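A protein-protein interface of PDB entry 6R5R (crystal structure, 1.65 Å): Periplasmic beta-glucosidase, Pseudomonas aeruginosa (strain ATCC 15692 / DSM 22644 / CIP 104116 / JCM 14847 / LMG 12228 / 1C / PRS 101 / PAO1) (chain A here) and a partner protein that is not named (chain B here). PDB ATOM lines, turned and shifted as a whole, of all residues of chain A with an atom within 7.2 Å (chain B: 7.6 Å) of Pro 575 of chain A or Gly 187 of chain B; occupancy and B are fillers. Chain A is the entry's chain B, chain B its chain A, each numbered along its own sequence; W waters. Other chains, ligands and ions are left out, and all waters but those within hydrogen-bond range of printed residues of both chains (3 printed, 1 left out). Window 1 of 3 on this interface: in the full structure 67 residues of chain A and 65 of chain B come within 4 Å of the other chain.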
ATOM      1  N   ARG A 131      12.578  26.249  16.644  1.00  0.00           N
ATOM      2  CA  ARG A 131      12.262  26.769  18.000  1.00  0.00           C
ATOM      3  C   ARG A 131      13.515  27.382  18.671  1.00  0.00           C
ATOM      4  O   ARG A 131      13.388  27.893  19.823  1.00  0.00           O
ATOM      5  CB  ARG A 131      11.718  25.662  18.889  1.00  0.00           C
ATOM      6  CG  ARG A 131      10.371  25.141  18.422  1.00  0.00           C
ATOM      7  CD  ARG A 131       9.954  23.948  19.258  1.00  0.00           C
ATOM      8  NE  ARG A 131       8.573  23.620  18.945  1.00  0.00           N
ATOM      9  CZ  ARG A 131       7.959  22.524  19.350  1.00  0.00           C
ATOM     10  NH1 ARG A 131       8.569  21.686  20.183  1.00  0.00           N
ATOM     11  NH2 ARG A 131       6.698  22.341  19.039  1.00  0.00           N
ATOM     12  N   ASP A 132      14.650  27.380  17.978  1.00  0.00           N
ATOM     13  CA  ASP A 132      15.938  27.843  18.542  1.00  0.00           C
ATOM     14  C   ASP A 132      16.471  28.961  17.672  1.00  0.00           C
ATOM     15  O   ASP A 132      17.009  28.743  16.614  1.00  0.00           O
ATOM     16  CB  ASP A 132      16.925  26.697  18.667  1.00  0.00           C
ATOM     17  CG  ASP A 132      18.181  27.047  19.464  1.00  0.00           C
ATOM     18  OD1 ASP A 132      18.630  28.218  19.426  1.00  0.00           O
ATOM     19  OD2 ASP A 132      18.624  26.127  20.203  1.00  0.00           O
ATOM     20  N   ALA A 133      16.271  30.199  18.141  1.00  0.00           N
ATOM     21  CA  ALA A 133      16.666  31.388  17.371  1.00  0.00           C
ATOM     22  C   ALA A 133      18.173  31.481  17.073  1.00  0.00           C
ATOM     23  O   ALA A 133      18.549  32.306  16.238  1.00  0.00           O
ATOM     24  CB  ALA A 133      16.193  32.601  18.163  1.00  0.00           C
ATOM     25  N   ARG A 134      19.030  30.723  17.745  1.00  0.00           N
ATOM     26  CA  ARG A 134      20.511  30.827  17.532  1.00  0.00           C
ATOM     27  C   ARG A 134      20.897  30.268  16.179  1.00  0.00           C
ATOM     28  O   ARG A 134      21.907  30.675  15.615  1.00  0.00           O
ATOM     29  CB  ARG A 134      21.253  30.042  18.611  1.00  0.00           C
ATOM     30  CG  ARG A 134      21.078  30.630  20.004  1.00  0.00           C
ATOM     31  CD  ARG A 134      21.713  29.702  21.006  1.00  0.00           C
ATOM     32  NE  ARG A 134      20.974  28.506  21.223  1.00  0.00           N
ATOM     33  CZ  ARG A 134      21.315  27.589  22.121  1.00  0.00           C
ATOM     34  NH1 ARG A 134      22.393  27.731  22.871  1.00  0.00           N
ATOM     35  NH2 ARG A 134      20.579  26.510  22.269  1.00  0.00           N
ATOM     36  N   ARG A 199       6.994  13.799  19.851  1.00  0.00           N
ATOM     37  CA  ARG A 199       7.322  15.188  19.428  1.00  0.00           C
ATOM     38  C   ARG A 199       7.622  15.202  17.916  1.00  0.00           C
ATOM     39  O   ARG A 199       7.200  16.113  17.180  1.00  0.00           O
ATOM     40  CB  ARG A 199       8.511  15.734  20.205  1.00  0.00           C
ATOM     41  CG  ARG A 199       8.966  17.099  19.725  1.00  0.00           C
ATOM     42  CD  ARG A 199      10.036  17.701  20.585  1.00  0.00           C
ATOM     43  NE  ARG A 199       9.470  18.241  21.816  1.00  0.00           N
ATOM     44  CZ  ARG A 199      10.130  19.061  22.650  1.00  0.00           C
ATOM     45  NH1 ARG A 199      11.385  19.370  22.447  1.00  0.00           N
ATOM     46  NH2 ARG A 199       9.545  19.531  23.714  1.00  0.00           N
ATOM     47  N   PRO A 568      12.672  35.976  21.836  1.00  0.00           N
ATOM     48  CA  PRO A 568      13.070  35.793  23.223  1.00  0.00           C
ATOM     49  C   PRO A 568      13.556  37.119  23.775  1.00  0.00           C
ATOM     50  O   PRO A 568      14.067  37.948  23.056  1.00  0.00           O
ATOM     51  CB  PRO A 568      14.270  34.849  23.205  1.00  0.00           C
ATOM     52  CG  PRO A 568      14.216  34.219  21.829  1.00  0.00           C
ATOM     53  CD  PRO A 568      13.572  35.249  20.920  1.00  0.00           C
ATOM     54  N   VAL A 571      19.073  35.376  24.771  1.00  0.00           N
ATOM     55  CA  VAL A 571      19.511  34.036  24.322  1.00  0.00           C
ATOM     56  C   VAL A 571      19.444  33.049  25.481  1.00  0.00           C
ATOM     57  O   VAL A 571      19.270  31.830  25.245  1.00  0.00           O
ATOM     58  CB  VAL A 571      20.916  34.113  23.715  1.00  0.00           C
ATOM     59  CG1 VAL A 571      22.006  34.332  24.767  1.00  0.00           C
ATOM     60  CG2 VAL A 571      21.224  32.843  22.906  1.00  0.00           C
ATOM     61  N   GLY A 572      19.558  33.532  26.717  1.00  0.00           N
ATOM     62  CA  GLY A 572      19.538  32.581  27.827  1.00  0.00           C
ATOM     63  C   GLY A 572      18.154  32.047  28.107  1.00  0.00           C
ATOM     64  O   GLY A 572      18.054  31.157  28.979  1.00  0.00           O
ATOM     65  N   GLN A 573      17.104  32.505  27.412  1.00  0.00           N
ATOM     66  CA  GLN A 573      15.744  31.921  27.506  1.00  0.00           C
ATOM     67  C   GLN A 573      15.493  30.853  26.438  1.00  0.00           C
ATOM     68  O   GLN A 573      14.416  30.247  26.447  1.00  0.00           O
ATOM     69  CB  GLN A 573      14.688  33.020  27.414  1.00  0.00           C
ATOM     70  CG  GLN A 573      14.894  34.070  28.488  1.00  0.00           C
ATOM     71  CD  GLN A 573      13.662  34.670  29.112  1.00  0.00           C
ATOM     72  OE1 GLN A 573      12.532  34.217  28.894  1.00  0.00           O
ATOM     73  NE2 GLN A 573      13.883  35.699  29.944  1.00  0.00           N
ATOM     74  N   VAL A 574      16.428  30.584  25.536  1.00  0.00           N
ATOM     75  CA  VAL A 574      16.127  29.658  24.414  1.00  0.00           C
ATOM     76  C   VAL A 574      15.956  28.253  24.963  1.00  0.00           C
ATOM     77  O   VAL A 574      16.717  27.794  25.829  1.00  0.00           O
ATOM     78  CB  VAL A 574      17.239  29.753  23.361  1.00  0.00           C
ATOM     79  CG1 VAL A 574      17.219  28.629  22.364  1.00  0.00           C
ATOM     80  CG2 VAL A 574      17.199  31.072  22.634  1.00  0.00           C
ATOM     81  N   PRO A 575      14.965  27.467  24.462  1.00  0.00           N
ATOM     82  CA  PRO A 575      13.970  27.890  23.479  1.00  0.00           C
ATOM     83  C   PRO A 575      12.736  28.530  24.114  1.00  0.00           C
ATOM     84  O   PRO A 575      12.285  28.150  25.173  1.00  0.00           O
ATOM     85  CB  PRO A 575      13.581  26.559  22.847  1.00  0.00           C
ATOM     86  CG  PRO A 575      13.606  25.604  24.038  1.00  0.00           C
ATOM     87  CD  PRO A 575      14.775  26.073  24.865  1.00  0.00           C
ATOM     88  N   VAL A 576      12.176  29.476  23.399  1.00  0.00           N
ATOM     89  CA  VAL A 576      10.834  29.989  23.754  1.00  0.00           C
ATOM     90  C   VAL A 576       9.973  29.834  22.513  1.00  0.00           C
ATOM     91  O   VAL A 576      10.381  30.189  21.410  1.00  0.00           O
ATOM     92  CB  VAL A 576      10.811  31.442  24.242  1.00  0.00           C
ATOM     93  CG1 VAL A 576      11.264  31.568  25.670  1.00  0.00           C
ATOM     94  CG2 VAL A 576      11.596  32.314  23.301  1.00  0.00           C
ATOM     95  N   TYR A 577       8.798  29.272  22.734  1.00  0.00           N
ATOM     96  CA  TYR A 577       7.830  29.081  21.634  1.00  0.00           C
ATOM     97  C   TYR A 577       6.448  29.007  22.237  1.00  0.00           C
ATOM     98  O   TYR A 577       6.324  28.616  23.405  1.00  0.00           O
ATOM     99  CB  TYR A 577       8.174  27.829  20.810  1.00  0.00           C
ATOM    100  CG  TYR A 577       8.372  26.573  21.607  1.00  0.00           C
ATOM    101  CD1 TYR A 577       9.596  26.283  22.197  1.00  0.00           C
ATOM    102  CD2 TYR A 577       7.353  25.658  21.765  1.00  0.00           C
ATOM    103  CE1 TYR A 577       9.805  25.094  22.866  1.00  0.00           C
ATOM    104  CE2 TYR A 577       7.547  24.458  22.428  1.00  0.00           C
ATOM    105  CZ  TYR A 577       8.791  24.147  22.959  1.00  0.00           C
ATOM    106  OH  TYR A 577       8.990  22.952  23.616  1.00  0.00           O
ATOM    107  N   HIS A 580       4.059  25.521  23.961  1.00  0.00           N
ATOM    108  CA  HIS A 580       4.786  24.776  25.001  1.00  0.00           C
ATOM    109  C   HIS A 580       3.794  24.053  25.894  1.00  0.00           C
ATOM    110  O   HIS A 580       2.593  24.349  25.913  1.00  0.00           O
ATOM    111  CB  HIS A 580       5.705  25.738  25.754  1.00  0.00           C
ATOM    112  CG  HIS A 580       4.975  26.829  26.468  1.00  0.00           C
ATOM    113  ND1 HIS A 580       4.880  28.110  25.920  1.00  0.00           N
ATOM    114  CD2 HIS A 580       4.212  26.844  27.587  1.00  0.00           C
ATOM    115  CE1 HIS A 580       4.135  28.858  26.719  1.00  0.00           C
ATOM    116  NE2 HIS A 580       3.729  28.125  27.724  1.00  0.00           N
ATOM    117  N   TYR A 599      12.701  31.906  34.951  1.00  0.00           N
ATOM    118  CA  TYR A 599      14.014  32.454  35.330  1.00  0.00           C
ATOM    119  C   TYR A 599      13.807  33.538  36.372  1.00  0.00           C
ATOM    120  O   TYR A 599      12.713  34.170  36.400  1.00  0.00           O
ATOM    121  CB  TYR A 599      14.689  33.107  34.127  1.00  0.00           C
ATOM    122  CG  TYR A 599      14.822  32.148  32.970  1.00  0.00           C
ATOM    123  CD1 TYR A 599      15.807  31.173  32.993  1.00  0.00           C
ATOM    124  CD2 TYR A 599      13.995  32.217  31.876  1.00  0.00           C
ATOM    125  CE1 TYR A 599      15.943  30.282  31.943  1.00  0.00           C
ATOM    126  CE2 TYR A 599      14.100  31.306  30.837  1.00  0.00           C
ATOM    127  CZ  TYR A 599      15.095  30.360  30.844  1.00  0.00           C
ATOM    128  OH  TYR A 599      15.173  29.429  29.819  1.00  0.00           O
ATOM    129  N   ASP B 133      22.973  21.355  31.334  1.00  0.00           N
ATOM    130  CA  ASP B 133      22.404  22.709  31.126  1.00  0.00           C
ATOM    131  C   ASP B 133      22.685  23.528  32.384  1.00  0.00           C
ATOM    132  O   ASP B 133      22.021  23.406  33.402  1.00  0.00           O
ATOM    133  CB  ASP B 133      20.919  22.678  30.759  1.00  0.00           C
ATOM    134  CG  ASP B 133      20.405  24.045  30.306  1.00  0.00           C
ATOM    135  OD1 ASP B 133      20.892  25.108  30.798  1.00  0.00           O
ATOM    136  OD2 ASP B 133      19.493  24.028  29.412  1.00  0.00           O
ATOM    137  N   ARG B 135      22.126  26.458  33.218  1.00  0.00           N
ATOM    138  CA  ARG B 135      21.128  27.462  33.673  1.00  0.00           C
ATOM    139  C   ARG B 135      20.288  26.952  34.832  1.00  0.00           C
ATOM    140  O   ARG B 135      19.758  27.756  35.620  1.00  0.00           O
ATOM    141  CB  ARG B 135      20.208  27.841  32.531  1.00  0.00           C
ATOM    142  CG  ARG B 135      20.914  28.516  31.379  1.00  0.00           C
ATOM    143  CD  ARG B 135      19.958  28.736  30.233  1.00  0.00           C
ATOM    144  NE  ARG B 135      19.666  27.500  29.544  1.00  0.00           N
ATOM    145  CZ  ARG B 135      18.944  27.443  28.437  1.00  0.00           C
ATOM    146  NH1 ARG B 135      18.390  28.541  27.927  1.00  0.00           N
ATOM    147  NH2 ARG B 135      18.729  26.269  27.861  1.00  0.00           N
ATOM    148  N   TRP B 136      20.120  25.646  34.876  1.00  0.00           N
ATOM    149  CA  TRP B 136      19.205  25.040  35.876  1.00  0.00           C
ATOM    150  C   TRP B 136      19.730  25.263  37.299  1.00  0.00           C
ATOM    151  O   TRP B 136      20.877  24.928  37.592  1.00  0.00           O
ATOM    152  CB  TRP B 136      19.038  23.579  35.532  1.00  0.00           C
ATOM    153  CG  TRP B 136      17.986  22.807  36.258  1.00  0.00           C
ATOM    154  CD1 TRP B 136      16.667  23.156  36.433  1.00  0.00           C
ATOM    155  CD2 TRP B 136      18.117  21.499  36.865  1.00  0.00           C
ATOM    156  NE1 TRP B 136      15.981  22.164  37.088  1.00  0.00           N
ATOM    157  CE2 TRP B 136      16.837  21.114  37.319  1.00  0.00           C
ATOM    158  CE3 TRP B 136      19.171  20.619  37.043  1.00  0.00           C
ATOM    159  CZ2 TRP B 136      16.587  19.886  37.928  1.00  0.00           C
ATOM    160  CZ3 TRP B 136      18.944  19.434  37.686  1.00  0.00           C
ATOM    161  CH2 TRP B 136      17.663  19.057  38.109  1.00  0.00           C
ATOM    162  N   ALA B 184      17.187  17.515  32.560  1.00  0.00           N
ATOM    163  CA  ALA B 184      17.158  17.848  31.117  1.00  0.00           C
ATOM    164  C   ALA B 184      16.033  18.824  30.799  1.00  0.00           C
ATOM    165  O   ALA B 184      15.725  19.039  29.593  1.00  0.00           O
ATOM    166  CB  ALA B 184      17.016  16.592  30.274  1.00  0.00           C
ATOM    167  N   ALA B 185      15.513  19.507  31.820  1.00  0.00           N
ATOM    168  CA  ALA B 185      14.463  20.522  31.626  1.00  0.00           C
ATOM    169  C   ALA B 185      14.786  21.435  30.447  1.00  0.00           C
ATOM    170  O   ALA B 185      15.882  22.088  30.399  1.00  0.00           O
ATOM    171  CB  ALA B 185      14.294  21.333  32.873  1.00  0.00           C
ATOM    172  N   GLU B 186      13.833  21.575  29.541  1.00  0.00           N
ATOM    173  CA  GLU B 186      14.015  22.482  28.394  1.00  0.00           C
ATOM    174  C   GLU B 186      14.243  23.914  28.873  1.00  0.00           C
ATOM    175  O   GLU B 186      13.542  24.415  29.797  1.00  0.00           O
ATOM    176  CB  GLU B 186      12.788  22.380  27.498  1.00  0.00           C
ATOM    177  CG  GLU B 186      13.021  22.740  26.086  1.00  0.00           C
ATOM    178  CD  GLU B 186      11.868  22.192  25.237  1.00  0.00           C
ATOM    179  OE1 GLU B 186      10.872  22.842  25.235  1.00  0.00           O
ATOM    180  OE2 GLU B 186      11.935  21.046  24.785  1.00  0.00           O
ATOM    181  N   GLY B 187      15.207  24.607  28.245  1.00  0.00           N
ATOM    182  CA  GLY B 187      15.531  25.988  28.625  1.00  0.00           C
ATOM    183  C   GLY B 187      16.209  26.112  29.965  1.00  0.00           C
ATOM    184  O   GLY B 187      16.466  27.232  30.395  1.00  0.00           O
ATOM    185  N   GLY B 188      16.550  25.002  30.612  1.00  0.00           N
ATOM    186  CA  GLY B 188      17.046  25.047  31.980  1.00  0.00           C
ATOM    187  C   GLY B 188      16.043  25.566  32.992  1.00  0.00           C
ATOM    188  O   GLY B 188      16.439  25.889  34.134  1.00  0.00           O
ATOM    189  N   ARG B 189      14.757  25.666  32.626  1.00  0.00           N
ATOM    190  CA  ARG B 189      13.705  26.187  33.515  1.00  0.00           C
ATOM    191  C   ARG B 189      13.265  25.057  34.409  1.00  0.00           C
ATOM    192  O   ARG B 189      12.933  23.961  33.924  1.00  0.00           O
ATOM    193  CB  ARG B 189      12.526  26.749  32.705  1.00  0.00           C
ATOM    194  CG  ARG B 189      12.885  27.977  31.917  1.00  0.00           C
ATOM    195  CD  ARG B 189      11.754  28.601  31.165  1.00  0.00           C
ATOM    196  NE  ARG B 189      11.254  27.901  29.999  1.00  0.00           N
ATOM    197  CZ  ARG B 189      11.694  28.004  28.713  1.00  0.00           C
ATOM    198  NH1 ARG B 189      12.785  28.674  28.351  1.00  0.00           N
ATOM    199  NH2 ARG B 189      11.022  27.357  27.765  1.00  0.00           N
ATOM    200  N   ASP B 190      13.240  25.326  35.704  1.00  0.00           N
ATOM    201  CA  ASP B 190      12.908  24.218  36.617  1.00  0.00           C
ATOM    202  C   ASP B 190      11.505  23.699  36.288  1.00  0.00           C
ATOM    203  O   ASP B 190      10.621  24.464  35.855  1.00  0.00           O
ATOM    204  CB  ASP B 190      13.051  24.641  38.059  1.00  0.00           C
ATOM    205  CG  ASP B 190      13.373  23.446  38.997  1.00  0.00           C
ATOM    206  OD1 ASP B 190      13.317  22.272  38.587  1.00  0.00           O
ATOM    207  OD2 ASP B 190      13.606  23.732  40.211  1.00  0.00           O
ATOM    208  N   ASN B 192      10.463  22.043  33.902  1.00  0.00           N
ATOM    209  CA  ASN B 192      10.006  22.118  32.510  1.00  0.00           C
ATOM    210  C   ASN B 192      10.157  20.759  31.814  1.00  0.00           C
ATOM    211  O   ASN B 192      10.908  19.849  32.237  1.00  0.00           O
ATOM    212  CB  ASN B 192      10.723  23.208  31.734  1.00  0.00           C
ATOM    213  CG  ASN B 192       9.958  23.660  30.515  1.00  0.00           C
ATOM    214  OD1 ASN B 192       8.739  23.469  30.422  1.00  0.00           O
ATOM    215  ND2 ASN B 192      10.653  24.276  29.572  1.00  0.00           N
ATOM    216  N   THR B 193       9.414  20.665  30.732  1.00  0.00           N
ATOM    217  CA  THR B 193       9.375  19.560  29.730  1.00  0.00           C
ATOM    218  C   THR B 193      10.740  18.943  29.493  1.00  0.00           C
ATOM    219  O   THR B 193      11.736  19.644  29.253  1.00  0.00           O
ATOM    220  CB  THR B 193       8.864  20.175  28.424  1.00  0.00           C
ATOM    221  OG1 THR B 193       7.612  20.799  28.715  1.00  0.00           O
ATOM    222  CG2 THR B 193       8.761  19.121  27.344  1.00  0.00           C
ATOM    223  N   SER B 490      16.400  29.421  38.056  1.00  0.00           N
ATOM    224  CA  SER B 490      17.111  29.257  36.770  1.00  0.00           C
ATOM    225  C   SER B 490      17.607  30.645  36.334  1.00  0.00           C
ATOM    226  O   SER B 490      16.949  31.692  36.572  1.00  0.00           O
ATOM    227  CB  SER B 490      16.217  28.608  35.784  1.00  0.00           C
ATOM    228  OG  SER B 490      15.770  27.299  36.253  1.00  0.00           O
ATOM    229  N   ARG B 491      18.773  30.652  35.753  1.00  0.00           N
ATOM    230  CA  ARG B 491      19.472  31.891  35.334  1.00  0.00           C
ATOM    231  C   ARG B 491      19.552  31.961  33.822  1.00  0.00           C
ATOM    232  O   ARG B 491      19.831  30.950  33.152  1.00  0.00           O
ATOM    233  CB  ARG B 491      20.900  31.892  35.870  1.00  0.00           C
ATOM    234  CG  ARG B 491      21.028  32.331  37.306  1.00  0.00           C
ATOM    235  CD  ARG B 491      22.439  32.630  37.778  1.00  0.00           C
ATOM    236  NE  ARG B 491      22.847  33.965  37.405  1.00  0.00           N
ATOM    237  CZ  ARG B 491      24.120  34.378  37.345  1.00  0.00           C
ATOM    238  NH1 ARG B 491      25.121  33.551  37.623  1.00  0.00           N
ATOM    239  NH2 ARG B 491      24.374  35.606  36.938  1.00  0.00           N
ATOM    240  N   THR B 492      19.372  33.169  33.297  1.00  0.00           N
ATOM    241  CA  THR B 492      19.555  33.466  31.868  1.00  0.00           C
ATOM    242  C   THR B 492      20.963  33.978  31.566  1.00  0.00           C
ATOM    243  O   THR B 492      21.237  34.269  30.401  1.00  0.00           O
ATOM    244  CB  THR B 492      18.542  34.509  31.359  1.00  0.00           C
ATOM    245  OG1 THR B 492      18.736  35.750  32.043  1.00  0.00           O
ATOM    246  CG2 THR B 492      17.108  34.052  31.515  1.00  0.00           C
ATOM    247  N   VAL B 572      26.206  31.691  28.139  1.00  0.00           N
ATOM    248  CA  VAL B 572      24.895  30.995  28.214  1.00  0.00           C
ATOM    249  C   VAL B 572      24.401  30.657  26.798  1.00  0.00           C
ATOM    250  O   VAL B 572      23.667  29.673  26.618  1.00  0.00           O
ATOM    251  CB  VAL B 572      23.887  31.825  28.996  1.00  0.00           C
ATOM    252  CG1 VAL B 572      23.406  33.058  28.234  1.00  0.00           C
ATOM    253  CG2 VAL B 572      22.700  30.985  29.387  1.00  0.00           C
ATOM    254  N   VAL B 575      24.865  26.952  25.482  1.00  0.00           N
ATOM    255  CA  VAL B 575      24.288  25.793  26.200  1.00  0.00           C
ATOM    256  C   VAL B 575      23.524  24.933  25.206  1.00  0.00           C
ATOM    257  O   VAL B 575      22.790  25.437  24.348  1.00  0.00           O
ATOM    258  CB  VAL B 575      23.416  26.287  27.363  1.00  0.00           C
ATOM    259  CG1 VAL B 575      22.521  25.213  27.908  1.00  0.00           C
ATOM    260  CG2 VAL B 575      24.264  26.893  28.471  1.00  0.00           C
HETATM  261  O   HOH W   1      19.858  27.065  25.129  1.00  0.00           O
HETATM  262  O   HOH W   2      20.955  29.576  25.623  1.00  0.00           O
HETATM  263  O   HOH W   3      20.935  35.839  28.256  1.00  0.00           O
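The side-chain amide nitrogen (ND2) of Asn 192 of chain B sits at hydrogen-bond distance from the backbone carbonyl oxygen (O) of Glu 186 of chain B.
The backbone carbonyl oxygen (O) of Arg 135 of chain B lies within hydrogen-bond range of the backbone NH (N) of Arg 491 of chain B (3.1 Å).
OD2 of Asp 132 of chain A is in salt-bridge range of NH2 of Arg 134 of chain A.
OH of Tyr 577 of chain A sits at hydrogen-bond distance from NH2 of Arg 199 of chain A (3.5 Å).
The backbone carbonyl oxygen (O) of Tyr 577 of chain A lies within hydrogen-bond range of a ring nitrogen (ND1) of His 580 of chain A (2.9 Å).
The guanidinium group of Arg 135 of chain B sits close to the backbone carbonyl oxygen of Gly 187 of chain B (3.3 Å).
Hydrophobic or aromatic side chains of chain A that line the printed part of chain B: Val 571, Pro 575, Tyr 577 and Tyr 599.
Of the 17 printed residues of chain B, 10 touch a printed residue of chain A.
Among the printed residues, 22 pairs touch across the chains.
Among the printed residues, Asp or Glu carboxylates within 4 Å of a Lys or Arg side-chain nitrogen of the other chain: Arg 199 of chain A with Glu 186 of chain B (2.9 Å).
Printed residues of chain B within 4 Å of Gln 573 of chain A: Arg 135, Arg 189 and Thr 492.
Pro 575 of chain A touches three residues of chain B.
Of the printed residues of chain B, Tyr 599 of chain A touches Arg 135, Gly 187, Arg 189, Ser 490, Arg 491 and Thr 492.
Of the printed residues of chain A, Glu 186 of chain B touches Arg 199, Pro 575 and Tyr 577.
Of chain A, only Val 574, Pro 575 and Tyr 599 come within 4 Å of Gly 187 of chain B.
Asp 190 of chain B touches none of the printed residues of chain A.
Of the printed residues of chain A, Thr 492 of chain B touches Gly 572 (3.5 Å), Gln 573 (3.8 Å) and Tyr 599 (3.3 Å).
Of the printed residues of chain A, Val 572 of chain B touches Val 571 and Gly 572.
The nearest residue of chain B that does not touch Pro 575 of chain A is Arg 135 of chain B (5.0 Å).
The nearest residue of chain A that does not touch Gly 187 of chain B is Gly 572 of chain A (4.5 Å).
Thr 193 of chain B touches Arg 199 of chain A (CG2 to NH2, 3.7 Å).
Val 572 of chain B touches Val 571 of chain A.
Gln 573 of chain A touches Arg 135 of chain B.
CG2 of Thr 492 of chain B touches CG of Gln 573 of chain A (3.8 Å).
Val 574 of chain A touches Gly 187 of chain B.
Glu 186 of chain B touches Pro 575 of chain A (CG to CG, 3.6 Å).
N of Gly 187 of chain B touches CD of Pro 575 of chain A, 3.7 Å away.
Tyr 599 of chain A touches Arg 135 of chain B (OH to NH1, 3.8 Å).
Tyr 599 of chain A touches Ser 490 of chain B (CA to O, 3.3 Å).
C of Arg 491 of chain B touches CD1 of Tyr 599 of chain A, at 3.9 Å.
The guanidinium group of Arg 135 of chain B sits at hydrogen-bond distance from the backbone carbonyl oxygen of Val 574 of chain A.
The backbone carbonyl oxygen (O) of Gly 572 of chain A lies within hydrogen-bond range of the guanidinium group (NH1) of Arg 135 of chain B (2.8 Å).
The backbone carbonyl oxygen (O) of Gln 573 of chain A is in hydrogen-bond range of the guanidinium group (NH1) of Arg 189 of chain B (3.0 Å).
NH1 of Arg 134 of chain A sits at hydrogen-bond distance from O of Val 575 of chain B, at 2.8 Å.
O of Pro 575 of chain A lies within hydrogen-bond range of NH2 of Arg 189 of chain B (3.0 Å).
The backbone carbonyl oxygen of Gly 187 of chain B is in hydrogen-bond range of the side-chain hydroxyl of Tyr 599 of chain A, at 2.6 Å.
The guanidinium group (NH1) of Arg 189 of chain B lies within hydrogen-bond range of the side-chain hydroxyl (OH) of Tyr 599 of chain A, 2.9 Å away.
The guanidinium group of Arg 199 of chain A is in salt-bridge range of the side-chain carboxylate of Glu 186 of chain B (2.9 Å).
The side-chain hydroxyl (OH) of Tyr 577 of chain A is in hydrogen-bond range of the side-chain carboxylate (OE1) of Glu 186 of chain B (2.5 Å).
Water W3 lies within hydrogen-bond range of O of Thr 492 of chain B (2.7 Å) and N of Gly 572 of chain A (3.1 Å).
Water W2 bridges O of Val 571 of chain A (2.8 Å) and O of Val 572 of chain B (2.9 Å).
Water W1 lies within hydrogen-bond range of NH2 of Arg 134 of chain A (3.0 Å), NH2 of Arg 135 of chain B (3.1 Å), O of Val 574 of chain A (3.3 Å) and O of Val 575 of chain B (3.4 Å).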
